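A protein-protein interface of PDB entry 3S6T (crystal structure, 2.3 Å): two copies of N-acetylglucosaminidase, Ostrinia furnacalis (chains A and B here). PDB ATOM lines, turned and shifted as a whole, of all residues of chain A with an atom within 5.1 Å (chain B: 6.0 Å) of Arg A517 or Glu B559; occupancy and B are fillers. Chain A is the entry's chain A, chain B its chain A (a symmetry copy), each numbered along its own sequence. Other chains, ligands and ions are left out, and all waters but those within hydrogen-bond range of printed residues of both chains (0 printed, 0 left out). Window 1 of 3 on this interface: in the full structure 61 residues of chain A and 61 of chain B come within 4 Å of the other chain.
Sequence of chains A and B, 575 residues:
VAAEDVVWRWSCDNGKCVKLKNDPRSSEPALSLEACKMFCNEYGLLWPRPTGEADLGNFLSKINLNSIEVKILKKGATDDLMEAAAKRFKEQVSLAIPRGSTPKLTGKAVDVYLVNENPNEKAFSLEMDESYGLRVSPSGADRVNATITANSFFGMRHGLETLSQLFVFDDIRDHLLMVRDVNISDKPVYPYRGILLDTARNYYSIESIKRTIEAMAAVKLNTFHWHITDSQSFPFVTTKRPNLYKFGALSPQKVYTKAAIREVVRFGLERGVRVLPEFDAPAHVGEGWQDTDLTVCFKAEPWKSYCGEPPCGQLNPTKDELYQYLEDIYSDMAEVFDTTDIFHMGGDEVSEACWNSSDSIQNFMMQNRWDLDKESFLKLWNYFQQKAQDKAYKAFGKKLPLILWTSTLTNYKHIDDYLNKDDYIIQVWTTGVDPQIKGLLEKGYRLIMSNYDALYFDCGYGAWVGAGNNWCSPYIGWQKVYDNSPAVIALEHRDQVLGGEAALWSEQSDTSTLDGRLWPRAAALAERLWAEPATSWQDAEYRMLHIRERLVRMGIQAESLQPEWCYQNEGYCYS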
ATOM      1  N   PHE A 457      27.614  31.680  13.239  1.00  0.00           N
ATOM      2  CA  PHE A 457      27.540  30.290  12.830  1.00  0.00           C
ATOM      3  C   PHE A 457      26.295  29.540  13.279  1.00  0.00           C
ATOM      4  O   PHE A 457      26.043  28.510  12.808  1.00  0.00           O
ATOM      5  CB  PHE A 457      28.815  29.547  13.184  1.00  0.00           C
ATOM      6  CG  PHE A 457      29.976  29.862  12.293  1.00  0.00           C
ATOM      7  CD1 PHE A 457      30.017  30.992  11.557  1.00  0.00           C
ATOM      8  CD2 PHE A 457      31.039  29.041  12.227  1.00  0.00           C
ATOM      9  CE1 PHE A 457      31.074  31.245  10.776  1.00  0.00           C
ATOM     10  CE2 PHE A 457      32.079  29.316  11.460  1.00  0.00           C
ATOM     11  CZ  PHE A 457      32.104  30.393  10.739  1.00  0.00           C
ATOM     12  N   ASP A 458      25.562  30.084  14.225  1.00  0.00           N
ATOM     13  CA  ASP A 458      24.295  29.559  14.673  1.00  0.00           C
ATOM     14  C   ASP A 458      23.135  29.757  13.704  1.00  0.00           C
ATOM     15  O   ASP A 458      22.194  29.036  13.733  1.00  0.00           O
ATOM     16  CB  ASP A 458      23.956  30.037  16.086  1.00  0.00           C
ATOM     17  CG  ASP A 458      23.884  31.539  16.221  1.00  0.00           C
ATOM     18  OD1 ASP A 458      24.775  32.239  15.811  1.00  0.00           O
ATOM     19  OD2 ASP A 458      22.931  32.010  16.780  1.00  0.00           O
ATOM     20  N   TYR A 461      18.993  27.713  11.195  1.00  0.00           N
ATOM     21  CA  TYR A 461      18.218  26.547  11.545  1.00  0.00           C
ATOM     22  C   TYR A 461      16.808  26.871  11.931  1.00  0.00           C
ATOM     23  O   TYR A 461      16.385  27.984  11.845  1.00  0.00           O
ATOM     24  CB  TYR A 461      18.893  25.758  12.632  1.00  0.00           C
ATOM     25  CG  TYR A 461      20.180  25.291  12.140  1.00  0.00           C
ATOM     26  CD1 TYR A 461      20.301  24.085  11.535  1.00  0.00           C
ATOM     27  CD2 TYR A 461      21.264  26.095  12.208  1.00  0.00           C
ATOM     28  CE1 TYR A 461      21.438  23.709  11.059  1.00  0.00           C
ATOM     29  CE2 TYR A 461      22.381  25.726  11.744  1.00  0.00           C
ATOM     30  CZ  TYR A 461      22.467  24.548  11.164  1.00  0.00           C
ATOM     31  OH  TYR A 461      23.634  24.194  10.708  1.00  0.00           O
ATOM     32  N   LEU A 504      29.708  30.781  17.664  1.00  0.00           N
ATOM     33  CA  LEU A 504      28.776  29.697  17.773  1.00  0.00           C
ATOM     34  C   LEU A 504      27.998  29.767  19.067  1.00  0.00           C
ATOM     35  O   LEU A 504      28.352  29.230  20.063  1.00  0.00           O
ATOM     36  CB  LEU A 504      29.432  28.334  17.589  1.00  0.00           C
ATOM     37  CG  LEU A 504      28.630  27.057  17.758  1.00  0.00           C
ATOM     38  CD1 LEU A 504      27.512  26.930  16.796  1.00  0.00           C
ATOM     39  CD2 LEU A 504      29.487  25.893  17.666  1.00  0.00           C
ATOM     40  N   GLN A 508      21.072  26.083  19.960  1.00  0.00           N
ATOM     41  CA  GLN A 508      20.839  24.965  19.102  1.00  0.00           C
ATOM     42  C   GLN A 508      22.070  24.203  18.702  1.00  0.00           C
ATOM     43  O   GLN A 508      22.163  23.790  17.599  1.00  0.00           O
ATOM     44  CB  GLN A 508      20.104  25.428  17.872  1.00  0.00           C
ATOM     45  CG  GLN A 508      18.775  25.938  18.168  1.00  0.00           C
ATOM     46  CD  GLN A 508      18.059  26.409  16.980  1.00  0.00           C
ATOM     47  OE1 GLN A 508      18.332  27.458  16.471  1.00  0.00           O
ATOM     48  NE2 GLN A 508      17.132  25.649  16.534  1.00  0.00           N
ATOM     49  N   SER A 509      23.018  24.074  19.595  1.00  0.00           N
ATOM     50  CA  SER A 509      24.230  23.358  19.315  1.00  0.00           C
ATOM     51  C   SER A 509      24.820  22.801  20.598  1.00  0.00           C
ATOM     52  O   SER A 509      24.644  23.347  21.627  1.00  0.00           O
ATOM     53  CB  SER A 509      25.195  24.255  18.559  1.00  0.00           C
ATOM     54  OG  SER A 509      26.494  23.768  18.523  1.00  0.00           O
ATOM     55  N   THR A 513      26.813  18.494  17.598  1.00  0.00           N
ATOM     56  CA  THR A 513      26.752  19.307  16.400  1.00  0.00           C
ATOM     57  C   THR A 513      27.868  20.268  16.166  1.00  0.00           C
ATOM     58  O   THR A 513      27.866  20.974  15.237  1.00  0.00           O
ATOM     59  CB  THR A 513      25.524  20.148  16.378  1.00  0.00           C
ATOM     60  OG1 THR A 513      25.534  20.995  17.490  1.00  0.00           O
ATOM     61  CG2 THR A 513      24.346  19.333  16.445  1.00  0.00           C
ATOM     62  N   LEU A 514      28.809  20.308  17.039  1.00  0.00           N
ATOM     63  CA  LEU A 514      29.858  21.238  16.885  1.00  0.00           C
ATOM     64  C   LEU A 514      30.865  21.169  15.724  1.00  0.00           C
ATOM     65  O   LEU A 514      31.249  22.176  15.237  1.00  0.00           O
ATOM     66  CB  LEU A 514      30.460  21.459  18.204  1.00  0.00           C
ATOM     67  CG  LEU A 514      31.909  21.450  18.188  1.00  0.00           C
ATOM     68  CD1 LEU A 514      32.276  22.723  18.824  1.00  0.00           C
ATOM     69  CD2 LEU A 514      32.193  20.238  18.983  1.00  0.00           C
ATOM     70  N   ASP A 515      31.254  19.984  15.303  1.00  0.00           N
ATOM     71  CA  ASP A 515      32.160  19.796  14.207  1.00  0.00           C
ATOM     72  C   ASP A 515      31.531  20.357  12.932  1.00  0.00           C
ATOM     73  O   ASP A 515      32.175  20.970  12.133  1.00  0.00           O
ATOM     74  CB  ASP A 515      32.445  18.314  13.991  1.00  0.00           C
ATOM     75  CG  ASP A 515      33.432  17.714  14.965  1.00  0.00           C
ATOM     76  OD1 ASP A 515      33.903  18.323  15.899  1.00  0.00           O
ATOM     77  OD2 ASP A 515      33.735  16.567  14.780  1.00  0.00           O
ATOM     78  N   GLY A 516      30.260  20.079  12.760  1.00  0.00           N
ATOM     79  CA  GLY A 516      29.519  20.585  11.648  1.00  0.00           C
ATOM     80  C   GLY A 516      29.341  22.076  11.610  1.00  0.00           C
ATOM     81  O   GLY A 516      29.472  22.630  10.600  1.00  0.00           O
ATOM     82  N   ARG A 517      29.020  22.684  12.736  1.00  0.00           N
ATOM     83  CA  ARG A 517      28.824  24.114  12.815  1.00  0.00           C
ATOM     84  C   ARG A 517      30.062  24.938  12.509  1.00  0.00           C
ATOM     85  O   ARG A 517      30.004  25.881  11.804  1.00  0.00           O
ATOM     86  CB  ARG A 517      28.360  24.506  14.210  1.00  0.00           C
ATOM     87  CG  ARG A 517      26.999  24.071  14.639  1.00  0.00           C
ATOM     88  CD  ARG A 517      25.990  24.657  13.759  1.00  0.00           C
ATOM     89  NE  ARG A 517      24.660  24.648  14.292  1.00  0.00           N
ATOM     90  CZ  ARG A 517      23.792  23.680  14.110  1.00  0.00           C
ATOM     91  NH1 ARG A 517      24.112  22.618  13.438  1.00  0.00           N
ATOM     92  NH2 ARG A 517      22.610  23.787  14.603  1.00  0.00           N
ATOM     93  N   LEU A 518      31.151  24.583  13.147  1.00  0.00           N
ATOM     94  CA  LEU A 518      32.440  25.172  12.969  1.00  0.00           C
ATOM     95  C   LEU A 518      33.208  24.907  11.674  1.00  0.00           C
ATOM     96  O   LEU A 518      33.765  25.797  11.121  1.00  0.00           O
ATOM     97  CB  LEU A 518      33.311  24.862  14.168  1.00  0.00           C
ATOM     98  CG  LEU A 518      32.854  25.307  15.534  1.00  0.00           C
ATOM     99  CD1 LEU A 518      33.932  25.036  16.484  1.00  0.00           C
ATOM    100  CD2 LEU A 518      32.546  26.710  15.490  1.00  0.00           C
ATOM    101  N   TRP A 519      33.229  23.672  11.219  1.00  0.00           N
ATOM    102  CA  TRP A 519      34.049  23.280  10.093  1.00  0.00           C
ATOM    103  C   TRP A 519      33.312  22.803   8.867  1.00  0.00           C
ATOM    104  O   TRP A 519      32.369  22.115   8.964  1.00  0.00           O
ATOM    105  CB  TRP A 519      35.082  22.285  10.553  1.00  0.00           C
ATOM    106  CG  TRP A 519      35.679  22.639  11.858  1.00  0.00           C
ATOM    107  CD1 TRP A 519      35.415  22.062  13.018  1.00  0.00           C
ATOM    108  CD2 TRP A 519      36.642  23.655  12.134  1.00  0.00           C
ATOM    109  NE1 TRP A 519      36.118  22.617  13.995  1.00  0.00           N
ATOM    110  CE2 TRP A 519      36.877  23.617  13.489  1.00  0.00           C
ATOM    111  CE3 TRP A 519      37.299  24.603  11.373  1.00  0.00           C
ATOM    112  CZ2 TRP A 519      37.766  24.453  14.105  1.00  0.00           C
ATOM    113  CZ3 TRP A 519      38.167  25.427  11.985  1.00  0.00           C
ATOM    114  CH2 TRP A 519      38.391  25.357  13.336  1.00  0.00           C
ATOM    115  N   ARG A 521      33.621  26.078   7.802  1.00  0.00           N
ATOM    116  CA  ARG A 521      33.383  27.494   7.696  1.00  0.00           C
ATOM    117  C   ARG A 521      34.391  28.383   8.418  1.00  0.00           C
ATOM    118  O   ARG A 521      34.686  29.424   7.932  1.00  0.00           O
ATOM    119  CB  ARG A 521      31.971  27.854   8.089  1.00  0.00           C
ATOM    120  CG  ARG A 521      30.898  27.443   7.123  1.00  0.00           C
ATOM    121  CD  ARG A 521      29.550  27.923   7.537  1.00  0.00           C
ATOM    122  NE  ARG A 521      29.113  27.415   8.817  1.00  0.00           N
ATOM    123  CZ  ARG A 521      28.106  27.887   9.499  1.00  0.00           C
ATOM    124  NH1 ARG A 521      27.392  28.856   9.049  1.00  0.00           N
ATOM    125  NH2 ARG A 521      27.813  27.369  10.624  1.00  0.00           N
ATOM    126  N   TYR B 461      21.136  24.986   3.406  1.00  0.00           N
ATOM    127  CA  TYR B 461      22.542  25.284   3.534  1.00  0.00           C
ATOM    128  C   TYR B 461      23.048  26.202   2.465  1.00  0.00           C
ATOM    129  O   TYR B 461      22.305  26.692   1.669  1.00  0.00           O
ATOM    130  CB  TYR B 461      23.358  24.022   3.575  1.00  0.00           C
ATOM    131  CG  TYR B 461      22.970  23.252   4.748  1.00  0.00           C
ATOM    132  CD1 TYR B 461      23.613  23.410   5.930  1.00  0.00           C
ATOM    133  CD2 TYR B 461      21.904  22.425   4.693  1.00  0.00           C
ATOM    134  CE1 TYR B 461      23.223  22.758   6.971  1.00  0.00           C
ATOM    135  CE2 TYR B 461      21.522  21.783   5.713  1.00  0.00           C
ATOM    136  CZ  TYR B 461      22.168  21.955   6.847  1.00  0.00           C
ATOM    137  OH  TYR B 461      21.757  21.269   7.874  1.00  0.00           O
ATOM    138  N   TYR B 475      15.834  26.189   5.523  1.00  0.00           N
ATOM    139  CA  TYR B 475      15.954  24.954   6.250  1.00  0.00           C
ATOM    140  C   TYR B 475      14.614  24.601   6.890  1.00  0.00           C
ATOM    141  O   TYR B 475      13.951  25.428   7.427  1.00  0.00           O
ATOM    142  CB  TYR B 475      17.049  25.107   7.294  1.00  0.00           C
ATOM    143  CG  TYR B 475      17.329  23.926   8.164  1.00  0.00           C
ATOM    144  CD1 TYR B 475      16.713  23.781   9.373  1.00  0.00           C
ATOM    145  CD2 TYR B 475      18.212  22.974   7.787  1.00  0.00           C
ATOM    146  CE1 TYR B 475      16.970  22.730  10.150  1.00  0.00           C
ATOM    147  CE2 TYR B 475      18.476  21.923   8.563  1.00  0.00           C
ATOM    148  CZ  TYR B 475      17.844  21.808   9.743  1.00  0.00           C
ATOM    149  OH  TYR B 475      18.065  20.769  10.524  1.00  0.00           O
ATOM    150  N   ASP B 515      23.890  12.071  10.657  1.00  0.00           N
ATOM    151  CA  ASP B 515      23.177  11.993  11.900  1.00  0.00           C
ATOM    152  C   ASP B 515      22.440  13.310  12.141  1.00  0.00           C
ATOM    153  O   ASP B 515      21.332  13.335  12.589  1.00  0.00           O
ATOM    154  CB  ASP B 515      24.140  11.760  13.060  1.00  0.00           C
ATOM    155  CG  ASP B 515      24.625  10.336  13.198  1.00  0.00           C
ATOM    156  OD1 ASP B 515      24.350   9.457  12.413  1.00  0.00           O
ATOM    157  OD2 ASP B 515      25.326  10.101  14.144  1.00  0.00           O
ATOM    158  N   GLY B 516      23.123  14.397  11.868  1.00  0.00           N
ATOM    159  CA  GLY B 516      22.549  15.700  11.985  1.00  0.00           C
ATOM    160  C   GLY B 516      21.423  16.001  11.036  1.00  0.00           C
ATOM    161  O   GLY B 516      20.486  16.555  11.437  1.00  0.00           O
ATOM    162  N   ARG B 517      21.567  15.635   9.778  1.00  0.00           N
ATOM    163  CA  ARG B 517      20.549  15.875   8.779  1.00  0.00           C
ATOM    164  C   ARG B 517      19.238  15.151   9.031  1.00  0.00           C
ATOM    165  O   ARG B 517      18.206  15.707   8.910  1.00  0.00           O
ATOM    166  CB  ARG B 517      21.043  15.441   7.407  1.00  0.00           C
ATOM    167  CG  ARG B 517      22.151  16.225   6.787  1.00  0.00           C
ATOM    168  CD  ARG B 517      21.728  17.608   6.583  1.00  0.00           C
ATOM    169  NE  ARG B 517      22.529  18.343   5.650  1.00  0.00           N
ATOM    170  CZ  ARG B 517      23.585  19.053   5.975  1.00  0.00           C
ATOM    171  NH1 ARG B 517      24.000  19.105   7.202  1.00  0.00           N
ATOM    172  NH2 ARG B 517      24.214  19.705   5.064  1.00  0.00           N
ATOM    173  N   TRP B 519      18.342  13.295  12.038  1.00  0.00           N
ATOM    174  CA  TRP B 519      17.815  13.284  13.386  1.00  0.00           C
ATOM    175  C   TRP B 519      17.969  14.562  14.171  1.00  0.00           C
ATOM    176  O   TRP B 519      18.956  15.190  14.108  1.00  0.00           O
ATOM    177  CB  TRP B 519      18.370  12.096  14.128  1.00  0.00           C
ATOM    178  CG  TRP B 519      18.407  10.870  13.302  1.00  0.00           C
ATOM    179  CD1 TRP B 519      19.483  10.330  12.756  1.00  0.00           C
ATOM    180  CD2 TRP B 519      17.314  10.033  12.927  1.00  0.00           C
ATOM    181  NE1 TRP B 519      19.173   9.236  12.076  1.00  0.00           N
ATOM    182  CE2 TRP B 519      17.837   9.029  12.146  1.00  0.00           C
ATOM    183  CE3 TRP B 519      15.951  10.055  13.155  1.00  0.00           C
ATOM    184  CZ2 TRP B 519      17.067   8.030  11.620  1.00  0.00           C
ATOM    185  CZ3 TRP B 519      15.198   9.074  12.629  1.00  0.00           C
ATOM    186  CH2 TRP B 519      15.749   8.078  11.865  1.00  0.00           C
ATOM    187  N   PRO B 520      16.948  14.989  14.870  1.00  0.00           N
ATOM    188  CA  PRO B 520      15.715  14.258  15.073  1.00  0.00           C
ATOM    189  C   PRO B 520      14.553  14.563  14.140  1.00  0.00           C
ATOM    190  O   PRO B 520      13.482  14.129  14.417  1.00  0.00           O
ATOM    191  CB  PRO B 520      15.336  14.716  16.456  1.00  0.00           C
ATOM    192  CG  PRO B 520      15.771  16.032  16.503  1.00  0.00           C
ATOM    193  CD  PRO B 520      16.978  16.172  15.725  1.00  0.00           C
ATOM    194  N   ARG B 548      15.136  13.290  21.121  1.00  0.00           N
ATOM    195  CA  ARG B 548      16.394  13.784  20.686  1.00  0.00           C
ATOM    196  C   ARG B 548      17.501  13.357  21.625  1.00  0.00           C
ATOM    197  O   ARG B 548      18.544  12.960  21.199  1.00  0.00           O
ATOM    198  CB  ARG B 548      16.292  15.288  20.585  1.00  0.00           C
ATOM    199  CG  ARG B 548      17.455  15.973  20.021  1.00  0.00           C
ATOM    200  CD  ARG B 548      18.584  16.137  20.999  1.00  0.00           C
ATOM    201  NE  ARG B 548      19.798  16.515  20.337  1.00  0.00           N
ATOM    202  CZ  ARG B 548      20.910  16.907  20.928  1.00  0.00           C
ATOM    203  NH1 ARG B 548      21.020  16.963  22.217  1.00  0.00           N
ATOM    204  NH2 ARG B 548      21.929  17.205  20.203  1.00  0.00           N
ATOM    205  N   GLN B 557      24.653  11.432  16.437  1.00  0.00           N
ATOM    206  CA  GLN B 557      25.008  12.823  16.605  1.00  0.00           C
ATOM    207  C   GLN B 557      23.856  13.699  16.143  1.00  0.00           C
ATOM    208  O   GLN B 557      23.965  14.407  15.206  1.00  0.00           O
ATOM    209  CB  GLN B 557      26.236  13.205  15.779  1.00  0.00           C
ATOM    210  CG  GLN B 557      27.446  12.424  15.932  1.00  0.00           C
ATOM    211  CD  GLN B 557      27.935  12.392  17.318  1.00  0.00           C
ATOM    212  OE1 GLN B 557      27.793  11.407  17.976  1.00  0.00           O
ATOM    213  NE2 GLN B 557      28.503  13.454  17.771  1.00  0.00           N
ATOM    214  N   ALA B 558      22.755  13.650  16.849  1.00  0.00           N
ATOM    215  CA  ALA B 558      21.567  14.385  16.494  1.00  0.00           C
ATOM    216  C   ALA B 558      21.677  15.875  16.667  1.00  0.00           C
ATOM    217  O   ALA B 558      22.387  16.335  17.493  1.00  0.00           O
ATOM    218  CB  ALA B 558      20.432  13.887  17.242  1.00  0.00           C
ATOM    219  N   GLU B 559      20.932  16.603  15.870  1.00  0.00           N
ATOM    220  CA  GLU B 559      20.864  18.028  15.929  1.00  0.00           C
ATOM    221  C   GLU B 559      20.292  18.454  17.242  1.00  0.00           C
ATOM    222  O   GLU B 559      19.492  17.783  17.828  1.00  0.00           O
ATOM    223  CB  GLU B 559      19.941  18.559  14.853  1.00  0.00           C
ATOM    224  CG  GLU B 559      20.569  18.940  13.588  1.00  0.00           C
ATOM    225  CD  GLU B 559      21.442  20.155  13.687  1.00  0.00           C
ATOM    226  OE1 GLU B 559      22.424  20.218  12.982  1.00  0.00           O
ATOM    227  OE2 GLU B 559      21.143  21.040  14.464  1.00  0.00           O
ATOM    228  N   SER B 560      20.707  19.605  17.692  1.00  0.00           N
ATOM    229  CA  SER B 560      20.178  20.151  18.903  1.00  0.00           C
ATOM    230  C   SER B 560      19.010  21.075  18.562  1.00  0.00           C
ATOM    231  O   SER B 560      19.117  21.909  17.717  1.00  0.00           O
ATOM    232  CB  SER B 560      21.281  20.838  19.669  1.00  0.00           C
ATOM    233  OG  SER B 560      20.800  21.704  20.623  1.00  0.00           O
ATOM    234  N   LEU B 561      17.870  20.833  19.170  1.00  0.00           N
ATOM    235  CA  LEU B 561      16.682  21.627  18.977  1.00  0.00           C
ATOM    236  C   LEU B 561      16.548  22.882  19.826  1.00  0.00           C
ATOM    237  O   LEU B 561      16.191  23.900  19.340  1.00  0.00           O
ATOM    238  CB  LEU B 561      15.465  20.745  19.158  1.00  0.00           C
ATOM    239  CG  LEU B 561      14.735  20.150  17.971  1.00  0.00           C
ATOM    240  CD1 LEU B 561      15.599  19.930  16.787  1.00  0.00           C
ATOM    241  CD2 LEU B 561      14.077  18.888  18.367  1.00  0.00           C
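The backbone carbonyl oxygen (O) of Leu B561 sits at hydrogen-bond distance from the side-chain amide nitrogen (NE2) of Gln A508 (3.4 Å).
N of Ser A509 is in hydrogen-bond range of OG of Ser B560.
NH1 of Arg A517 lies within salt-bridge range of OE1 of Glu B559 (3.0 Å).
OH of Tyr A461 sits at hydrogen-bond distance from NH1 of Arg A517 (3.2 Å).
NH2 of Arg A517 is in hydrogen-bond range of O of Gln A508 (3.0 Å).
The side-chain hydroxyl (OG) of Ser A509 sits at hydrogen-bond distance from the side-chain hydroxyl (OG1) of Thr A513 (3.1 Å).
The backbone carbonyl oxygen of Trp B519 lies within hydrogen-bond range of the backbone NH of Glu B559, at 3.0 Å.
NH2 of Arg B548 sits at hydrogen-bond distance from O of Ala B558 (2.9 Å).
NE of Arg B548 lies within hydrogen-bond range of O of Glu B559 (2.8 Å).
Among the printed residues, pairs that only touch across the chains: Gln A508 with Ser B560 (3.4 Å), Thr A513 with Ala B558 (3.7 Å), Thr A513 with Glu B559 (3.8 Å), Tyr A461 with Tyr B475 (3.8 Å) and Thr A513 with Ser B560 (3.9 Å).
Of the printed residues of chain B, Tyr A461 touches Tyr B475.
Arg A517 touches just one residue of chain B: Glu B559.
Of the printed residues of chain A, Ser B560 touches Gln A508, Ser A509 and Thr A513.
Of the printed residues of chain A, Leu B561 touches Gln A508 (3.4 Å).
The nearest residue of chain B that does not touch Arg A517 is Ser B560 (5.0 Å).
The nearest printed residue of chain A that does not touch Leu B561 is Ser A509 (6.1 Å).
Printed residues of chain A that touch a printed residue of chain B: Tyr A461, Gln A508, Ser A509, Thr A513 and Arg A517.
Hydrophobic or aromatic side chains of chain A within 4 Å of the printed part of chain B: Tyr A461.
Hydrophobic or aromatic side chains of chain B within 4 Å of the printed part of chain A: Tyr B475.
Among the printed residues, Asp or Glu carboxylates within 4 Å of a Lys or Arg side-chain nitrogen of the other chain: Arg A517 with Glu B559 (3.0 Å).
Positions printed for both chains: 461, 515, 516, 517 and 519.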
